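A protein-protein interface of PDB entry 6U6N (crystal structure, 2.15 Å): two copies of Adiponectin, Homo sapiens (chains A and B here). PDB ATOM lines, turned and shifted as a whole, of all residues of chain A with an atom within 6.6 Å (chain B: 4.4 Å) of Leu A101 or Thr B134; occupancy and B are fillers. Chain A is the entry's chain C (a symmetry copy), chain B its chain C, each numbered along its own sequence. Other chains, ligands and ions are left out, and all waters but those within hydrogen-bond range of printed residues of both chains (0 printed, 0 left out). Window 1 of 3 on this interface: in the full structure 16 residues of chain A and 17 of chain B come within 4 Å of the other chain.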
ATOM      1  N   LEU A  56      35.489  29.693 -14.678  1.00  0.00           N
ATOM      2  CA  LEU A  56      34.058  29.453 -14.560  1.00  0.00           C
ATOM      3  C   LEU A  56      33.661  29.411 -13.091  1.00  0.00           C
ATOM      4  O   LEU A  56      34.239  28.652 -12.306  1.00  0.00           O
ATOM      5  CB  LEU A  56      33.676  28.141 -15.247  1.00  0.00           C
ATOM      6  CG  LEU A  56      32.201  27.740 -15.173  1.00  0.00           C
ATOM      7  CD1 LEU A  56      31.327  28.787 -15.848  1.00  0.00           C
ATOM      8  CD2 LEU A  56      31.987  26.368 -15.795  1.00  0.00           C
ATOM      9  N   TYR A  57      32.671  30.222 -12.728  1.00  0.00           N
ATOM     10  CA  TYR A  57      32.224  30.358 -11.350  1.00  0.00           C
ATOM     11  C   TYR A  57      30.765  29.946 -11.229  1.00  0.00           C
ATOM     12  O   TYR A  57      29.959  30.208 -12.128  1.00  0.00           O
ATOM     13  CB  TYR A  57      32.400  31.797 -10.853  1.00  0.00           C
ATOM     14  CG  TYR A  57      33.837  32.170 -10.577  1.00  0.00           C
ATOM     15  CD1 TYR A  57      34.714  32.454 -11.615  1.00  0.00           C
ATOM     16  CD2 TYR A  57      34.316  32.239  -9.277  1.00  0.00           C
ATOM     17  CE1 TYR A  57      36.028  32.792 -11.366  1.00  0.00           C
ATOM     18  CE2 TYR A  57      35.628  32.578  -9.017  1.00  0.00           C
ATOM     19  CZ  TYR A  57      36.480  32.852 -10.063  1.00  0.00           C
ATOM     20  OH  TYR A  57      37.788  33.191  -9.802  1.00  0.00           O
ATOM     21  N   TYR A  58      30.432  29.303 -10.115  1.00  0.00           N
ATOM     22  CA  TYR A  58      29.067  28.908  -9.801  1.00  0.00           C
ATOM     23  C   TYR A  58      28.519  29.837  -8.728  1.00  0.00           C
ATOM     24  O   TYR A  58      29.138  30.003  -7.673  1.00  0.00           O
ATOM     25  CB  TYR A  58      29.016  27.454  -9.329  1.00  0.00           C
ATOM     26  CG  TYR A  58      27.627  26.943  -9.019  1.00  0.00           C
ATOM     27  CD1 TYR A  58      26.742  26.625 -10.040  1.00  0.00           C
ATOM     28  CD2 TYR A  58      27.209  26.761  -7.707  1.00  0.00           C
ATOM     29  CE1 TYR A  58      25.472  26.149  -9.763  1.00  0.00           C
ATOM     30  CE2 TYR A  58      25.943  26.285  -7.419  1.00  0.00           C
ATOM     31  CZ  TYR A  58      25.078  25.980  -8.450  1.00  0.00           C
ATOM     32  OH  TYR A  58      23.817  25.505  -8.168  1.00  0.00           O
ATOM     33  N   PHE A  59      27.373  30.452  -9.004  1.00  0.00           N
ATOM     34  CA  PHE A  59      26.711  31.347  -8.064  1.00  0.00           C
ATOM     35  C   PHE A  59      25.333  30.800  -7.727  1.00  0.00           C
ATOM     36  O   PHE A  59      24.596  30.360  -8.614  1.00  0.00           O
ATOM     37  CB  PHE A  59      26.579  32.764  -8.631  1.00  0.00           C
ATOM     38  CG  PHE A  59      27.888  33.468  -8.812  1.00  0.00           C
ATOM     39  CD1 PHE A  59      28.539  33.446 -10.033  1.00  0.00           C
ATOM     40  CD2 PHE A  59      28.470  34.154  -7.758  1.00  0.00           C
ATOM     41  CE1 PHE A  59      29.747  34.094 -10.202  1.00  0.00           C
ATOM     42  CE2 PHE A  59      29.678  34.805  -7.920  1.00  0.00           C
ATOM     43  CZ  PHE A  59      30.318  34.774  -9.142  1.00  0.00           C
ATOM     44  N   SER A  99      20.423  29.810  -9.309  1.00  0.00           N
ATOM     45  CA  SER A  99      21.821  29.434  -9.429  1.00  0.00           C
ATOM     46  C   SER A  99      22.193  29.460 -10.904  1.00  0.00           C
ATOM     47  O   SER A  99      21.347  29.231 -11.771  1.00  0.00           O
ATOM     48  CB  SER A  99      22.098  28.054  -8.822  1.00  0.00           C
ATOM     49  OG  SER A  99      21.444  27.030  -9.549  1.00  0.00           O
ATOM     50  N   VAL A 100      23.467  29.743 -11.178  1.00  0.00           N
ATOM     51  CA  VAL A 100      23.921  29.946 -12.548  1.00  0.00           C
ATOM     52  C   VAL A 100      25.433  29.781 -12.582  1.00  0.00           C
ATOM     53  O   VAL A 100      26.118  29.983 -11.576  1.00  0.00           O
ATOM     54  CB  VAL A 100      23.482  31.339 -13.070  1.00  0.00           C
ATOM     55  CG1 VAL A 100      24.248  32.442 -12.357  1.00  0.00           C
ATOM     56  CG2 VAL A 100      23.662  31.438 -14.572  1.00  0.00           C
ATOM     57  N   LEU A 101      25.952  29.394 -13.746  1.00  0.00           N
ATOM     58  CA  LEU A 101      27.385  29.381 -14.009  1.00  0.00           C
ATOM     59  C   LEU A 101      27.749  30.614 -14.823  1.00  0.00           C
ATOM     60  O   LEU A 101      27.078  30.932 -15.810  1.00  0.00           O
ATOM     61  CB  LEU A 101      27.802  28.117 -14.762  1.00  0.00           C
ATOM     62  CG  LEU A 101      27.813  26.790 -14.002  1.00  0.00           C
ATOM     63  CD1 LEU A 101      27.944  25.627 -14.974  1.00  0.00           C
ATOM     64  CD2 LEU A 101      28.942  26.766 -12.988  1.00  0.00           C
ATOM     65  N   LEU A 102      28.808  31.305 -14.407  1.00  0.00           N
ATOM     66  CA  LEU A 102      29.280  32.494 -15.102  1.00  0.00           C
ATOM     67  C   LEU A 102      30.794  32.435 -15.221  1.00  0.00           C
ATOM     68  O   LEU A 102      31.484  32.110 -14.249  1.00  0.00           O
ATOM     69  CB  LEU A 102      28.868  33.777 -14.369  1.00  0.00           C
ATOM     70  CG  LEU A 102      27.376  34.081 -14.240  1.00  0.00           C
ATOM     71  CD1 LEU A 102      27.164  35.324 -13.397  1.00  0.00           C
ATOM     72  CD2 LEU A 102      26.742  34.254 -15.608  1.00  0.00           C
ATOM     73  N   HIS A 103      31.304  32.750 -16.406  1.00  0.00           N
ATOM     74  CA  HIS A 103      32.738  32.873 -16.617  1.00  0.00           C
ATOM     75  C   HIS A 103      33.168  34.302 -16.314  1.00  0.00           C
ATOM     76  O   HIS A 103      32.552  35.259 -16.794  1.00  0.00           O
ATOM     77  CB  HIS A 103      33.118  32.494 -18.049  1.00  0.00           C
ATOM     78  CG  HIS A 103      34.595  32.409 -18.271  1.00  0.00           C
ATOM     79  ND1 HIS A 103      35.357  33.496 -18.641  1.00  0.00           N
ATOM     80  CD2 HIS A 103      35.453  31.367 -18.166  1.00  0.00           C
ATOM     81  CE1 HIS A 103      36.620  33.127 -18.758  1.00  0.00           C
ATOM     82  NE2 HIS A 103      36.706  31.840 -18.475  1.00  0.00           N
ATOM     83  N   PHE A 136      31.682  30.266  -5.996  1.00  0.00           N
ATOM     84  CA  PHE A 136      32.991  29.639  -5.892  1.00  0.00           C
ATOM     85  C   PHE A 136      33.533  29.332  -7.280  1.00  0.00           C
ATOM     86  O   PHE A 136      32.773  29.149  -8.235  1.00  0.00           O
ATOM     87  CB  PHE A 136      32.945  28.362  -5.039  1.00  0.00           C
ATOM     88  CG  PHE A 136      31.962  27.326  -5.521  1.00  0.00           C
ATOM     89  CD1 PHE A 136      32.334  26.382  -6.464  1.00  0.00           C
ATOM     90  CD2 PHE A 136      30.677  27.277  -5.003  1.00  0.00           C
ATOM     91  CE1 PHE A 136      31.438  25.422  -6.897  1.00  0.00           C
ATOM     92  CE2 PHE A 136      29.777  26.318  -5.432  1.00  0.00           C
ATOM     93  CZ  PHE A 136      30.158  25.390  -6.381  1.00  0.00           C
ATOM     94  N   LEU A 138      34.790  27.103  -9.977  1.00  0.00           N
ATOM     95  CA  LEU A 138      34.682  25.701 -10.367  1.00  0.00           C
ATOM     96  C   LEU A 138      35.860  25.279 -11.241  1.00  0.00           C
ATOM     97  O   LEU A 138      36.624  24.380 -10.875  1.00  0.00           O
ATOM     98  CB  LEU A 138      33.356  25.460 -11.095  1.00  0.00           C
ATOM     99  CG  LEU A 138      33.123  24.027 -11.572  1.00  0.00           C
ATOM    100  CD1 LEU A 138      32.977  23.081 -10.387  1.00  0.00           C
ATOM    101  CD2 LEU A 138      31.908  23.968 -12.478  1.00  0.00           C
ATOM    102  N   ALA B  13      30.420  21.261 -18.199  1.00  0.00           N
ATOM    103  CA  ALA B  13      29.457  22.041 -17.440  1.00  0.00           C
ATOM    104  C   ALA B  13      28.505  22.722 -18.410  1.00  0.00           C
ATOM    105  O   ALA B  13      28.762  22.797 -19.613  1.00  0.00           O
ATOM    106  CB  ALA B  13      30.155  23.074 -16.546  1.00  0.00           C
ATOM    107  N   PHE B  14      27.397  23.222 -17.865  1.00  0.00           N
ATOM    108  CA  PHE B  14      26.414  23.982 -18.628  1.00  0.00           C
ATOM    109  C   PHE B  14      25.488  24.692 -17.653  1.00  0.00           C
ATOM    110  O   PHE B  14      25.254  24.211 -16.539  1.00  0.00           O
ATOM    111  CB  PHE B  14      25.602  23.082 -19.573  1.00  0.00           C
ATOM    112  CG  PHE B  14      24.583  22.223 -18.871  1.00  0.00           C
ATOM    113  CD1 PHE B  14      24.949  21.013 -18.309  1.00  0.00           C
ATOM    114  CD2 PHE B  14      23.258  22.625 -18.778  1.00  0.00           C
ATOM    115  CE1 PHE B  14      24.016  20.219 -17.662  1.00  0.00           C
ATOM    116  CE2 PHE B  14      22.321  21.836 -18.131  1.00  0.00           C
ATOM    117  CZ  PHE B  14      22.702  20.631 -17.572  1.00  0.00           C
ATOM    118  N   SER B  15      24.967  25.838 -18.085  1.00  0.00           N
ATOM    119  CA  SER B  15      23.956  26.574 -17.332  1.00  0.00           C
ATOM    120  C   SER B  15      23.082  27.308 -18.338  1.00  0.00           C
ATOM    121  O   SER B  15      23.591  28.104 -19.133  1.00  0.00           O
ATOM    122  CB  SER B  15      24.593  27.553 -16.346  1.00  0.00           C
ATOM    123  OG  SER B  15      23.610  28.148 -15.517  1.00  0.00           O
ATOM    124  N   PHE B  35      23.746  30.498 -20.524  1.00  0.00           N
ATOM    125  CA  PHE B  35      24.698  31.224 -19.690  1.00  0.00           C
ATOM    126  C   PHE B  35      26.112  30.693 -19.875  1.00  0.00           C
ATOM    127  O   PHE B  35      27.073  31.470 -19.901  1.00  0.00           O
ATOM    128  CB  PHE B  35      24.291  31.142 -18.217  1.00  0.00           C
ATOM    129  CG  PHE B  35      22.924  31.696 -17.929  1.00  0.00           C
ATOM    130  CD1 PHE B  35      21.850  30.846 -17.716  1.00  0.00           C
ATOM    131  CD2 PHE B  35      22.711  33.065 -17.863  1.00  0.00           C
ATOM    132  CE1 PHE B  35      20.592  31.347 -17.449  1.00  0.00           C
ATOM    133  CE2 PHE B  35      21.452  33.573 -17.596  1.00  0.00           C
ATOM    134  CZ  PHE B  35      20.392  32.713 -17.389  1.00  0.00           C
ATOM    135  N   TYR B  36      26.256  29.377 -20.006  1.00  0.00           N
ATOM    136  CA  TYR B  36      27.552  28.751 -20.216  1.00  0.00           C
ATOM    137  C   TYR B  36      27.362  27.441 -20.965  1.00  0.00           C
ATOM    138  O   TYR B  36      26.463  26.658 -20.646  1.00  0.00           O
ATOM    139  CB  TYR B  36      28.277  28.489 -18.892  1.00  0.00           C
ATOM    140  CG  TYR B  36      29.616  27.805 -19.061  1.00  0.00           C
ATOM    141  CD1 TYR B  36      29.732  26.425 -18.963  1.00  0.00           C
ATOM    142  CD2 TYR B  36      30.761  28.543 -19.328  1.00  0.00           C
ATOM    143  CE1 TYR B  36      30.953  25.799 -19.122  1.00  0.00           C
ATOM    144  CE2 TYR B  36      31.984  27.926 -19.486  1.00  0.00           C
ATOM    145  CZ  TYR B  36      32.075  26.554 -19.382  1.00  0.00           C
ATOM    146  OH  TYR B  36      33.295  25.936 -19.541  1.00  0.00           O
ATOM    147  N   TYR B  58      26.816  17.337 -10.556  1.00  0.00           N
ATOM    148  CA  TYR B  58      25.888  18.096  -9.731  1.00  0.00           C
ATOM    149  C   TYR B  58      24.909  18.829 -10.636  1.00  0.00           C
ATOM    150  O   TYR B  58      25.325  19.557 -11.542  1.00  0.00           O
ATOM    151  CB  TYR B  58      26.638  19.088  -8.840  1.00  0.00           C
ATOM    152  CG  TYR B  58      25.753  19.893  -7.915  1.00  0.00           C
ATOM    153  CD1 TYR B  58      25.199  19.318  -6.780  1.00  0.00           C
ATOM    154  CD2 TYR B  58      25.490  21.234  -8.166  1.00  0.00           C
ATOM    155  CE1 TYR B  58      24.395  20.053  -5.926  1.00  0.00           C
ATOM    156  CE2 TYR B  58      24.690  21.978  -7.319  1.00  0.00           C
ATOM    157  CZ  TYR B  58      24.145  21.383  -6.200  1.00  0.00           C
ATOM    158  OH  TYR B  58      23.348  22.120  -5.352  1.00  0.00           O
ATOM    159  N   PHE B  59      23.616  18.622 -10.404  1.00  0.00           N
ATOM    160  CA  PHE B  59      22.562  19.276 -11.167  1.00  0.00           C
ATOM    161  C   PHE B  59      21.707  20.118 -10.235  1.00  0.00           C
ATOM    162  O   PHE B  59      21.341  19.672  -9.143  1.00  0.00           O
ATOM    163  CB  PHE B  59      21.680  18.259 -11.899  1.00  0.00           C
ATOM    164  CG  PHE B  59      22.391  17.513 -12.986  1.00  0.00           C
ATOM    165  CD1 PHE B  59      22.961  16.276 -12.737  1.00  0.00           C
ATOM    166  CD2 PHE B  59      22.490  18.049 -14.259  1.00  0.00           C
ATOM    167  CE1 PHE B  59      23.617  15.587 -13.738  1.00  0.00           C
ATOM    168  CE2 PHE B  59      23.145  17.366 -15.265  1.00  0.00           C
ATOM    169  CZ  PHE B  59      23.710  16.133 -15.004  1.00  0.00           C
ATOM    170  N   ALA B  60      21.390  21.335 -10.670  1.00  0.00           N
ATOM    171  CA  ALA B  60      20.563  22.252  -9.899  1.00  0.00           C
ATOM    172  C   ALA B  60      19.632  22.992 -10.846  1.00  0.00           C
ATOM    173  O   ALA B  60      20.026  23.348 -11.960  1.00  0.00           O
ATOM    174  CB  ALA B  60      21.415  23.252  -9.107  1.00  0.00           C
ATOM    175  N   THR B 132      16.146  28.275 -14.538  1.00  0.00           N
ATOM    176  CA  THR B 132      17.492  27.824 -14.851  1.00  0.00           C
ATOM    177  C   THR B 132      17.630  26.314 -14.713  1.00  0.00           C
ATOM    178  O   THR B 132      16.804  25.635 -14.097  1.00  0.00           O
ATOM    179  CB  THR B 132      18.527  28.510 -13.955  1.00  0.00           C
ATOM    180  OG1 THR B 132      17.993  28.672 -12.634  1.00  0.00           O
ATOM    181  CG2 THR B 132      18.908  29.858 -14.530  1.00  0.00           C
ATOM    182  N   PHE B 133      18.712  25.807 -15.300  1.00  0.00           N
ATOM    183  CA  PHE B 133      19.042  24.387 -15.276  1.00  0.00           C
ATOM    184  C   PHE B 133      20.552  24.295 -15.441  1.00  0.00           C
ATOM    185  O   PHE B 133      21.078  24.630 -16.506  1.00  0.00           O
ATOM    186  CB  PHE B 133      18.304  23.631 -16.381  1.00  0.00           C
ATOM    187  CG  PHE B 133      18.647  22.168 -16.459  1.00  0.00           C
ATOM    188  CD1 PHE B 133      18.863  21.427 -15.309  1.00  0.00           C
ATOM    189  CD2 PHE B 133      18.730  21.530 -17.687  1.00  0.00           C
ATOM    190  CE1 PHE B 133      19.174  20.079 -15.384  1.00  0.00           C
ATOM    191  CE2 PHE B 133      19.037  20.184 -17.768  1.00  0.00           C
ATOM    192  CZ  PHE B 133      19.261  19.457 -16.614  1.00  0.00           C
ATOM    193  N   THR B 134      21.245  23.864 -14.389  1.00  0.00           N
ATOM    194  CA  THR B 134      22.700  23.895 -14.344  1.00  0.00           C
ATOM    195  C   THR B 134      23.241  22.525 -13.968  1.00  0.00           C
ATOM    196  O   THR B 134      22.679  21.839 -13.107  1.00  0.00           O
ATOM    197  CB  THR B 134      23.197  24.948 -13.339  1.00  0.00           C
ATOM    198  OG1 THR B 134      22.690  26.237 -13.706  1.00  0.00           O
ATOM    199  CG2 THR B 134      24.716  25.005 -13.321  1.00  0.00           C
ATOM    200  N   GLY B 135      24.325  22.131 -14.617  1.00  0.00           N
ATOM    201  CA  GLY B 135      25.006  20.892 -14.282  1.00  0.00           C
ATOM    202  C   GLY B 135      26.484  21.021 -14.561  1.00  0.00           C
ATOM    203  O   GLY B 135      26.898  21.729 -15.486  1.00  0.00           O
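The side-chain hydroxyl (OG) of Ser B15 is in hydrogen-bond range of the backbone NH (N) of Leu A101 (3.2 Å).
The backbone carbonyl oxygen of Leu A56 is in hydrogen-bond range of the backbone NH of Leu A138 (2.9 Å). The backbone carbonyl oxygen of Ala B60 sits at hydrogen-bond distance from the backbone NH of Thr B134, 2.8 Å away. The backbone carbonyl oxygen (O) of Ser B15 is in hydrogen-bond range of the backbone NH (N) of Phe B35 (2.8 Å). The backbone carbonyl oxygen (O) of Phe A59 lies within hydrogen-bond range of the backbone NH (N) of Val A100, at 2.9 Å. The backbone carbonyl oxygen (O) of Phe A136 sits at hydrogen-bond distance from the backbone NH (N) of Tyr A58 (3.0 Å). The backbone carbonyl oxygen (O) of Tyr B36 lies within hydrogen-bond range of the backbone NH (N) of Ser B15, at 3.1 Å.
CD2 of Leu A56 touches CB of Ala B13, 3.8 Å away. Leu A56 touches Tyr B36 (CD2 to CE1, 3.5 Å). OH of Tyr A58 touches CE2 of Tyr B58, at 3.7 Å. Tyr A58 touches Ala B60. CE1 of Tyr A58 touches CG2 of Thr B134, 3.8 Å away. Ser A99 touches Ala B60 (OG to CB, 3.8 Å). Leu A101 touches Ala B13. Leu A101 touches Phe B14. Leu A101 touches Phe B35. Thr B134 touches Leu A101 (CG2 to CG, 3.6 Å).
Leu A101 touches just these residues of chain B: Ala B13 (3.7 Å), Phe B14 (3.4 Å), Ser B15 (3.2 Å), Phe B35 (3.7 Å) and Thr B134 (3.6 Å). Of chain A, only Tyr A58 (3.8 Å), Ser A99 (3.8 Å) and Leu A101 (3.6 Å) come within 4 Å of Thr B134. Of the printed residues of chain A, Tyr B36 touches Leu A56 (3.5 Å). Of the printed residues of chain A, Thr B132 touches Ser A99. Printed residues of chain A within 4 Å of Phe B14: Leu A101 (3.4 Å). Phe A136 touches none of the printed residues of chain B. The nearest residue of chain B that does not touch Leu A101 is Gly B135 (4.1 Å).
Hydrophobic or aromatic side chains of chain A that line the printed part of chain B: Leu A56, Tyr A58, Val A100 and Leu A101. Along chain A the printed residues that touch a printed residue of chain B span positions 56 to 101. Of the 12 printed residues of chain B, 9 touch a printed residue of chain A. Hydrophobic or aromatic side chains of chain B that line the printed part of chain A: Ala B13, Phe B35, Tyr B36, Tyr B58 and Ala B60.
Tyr B58 touches its own counterpart, Tyr A58. Positions printed for both chains: 58 and 59.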
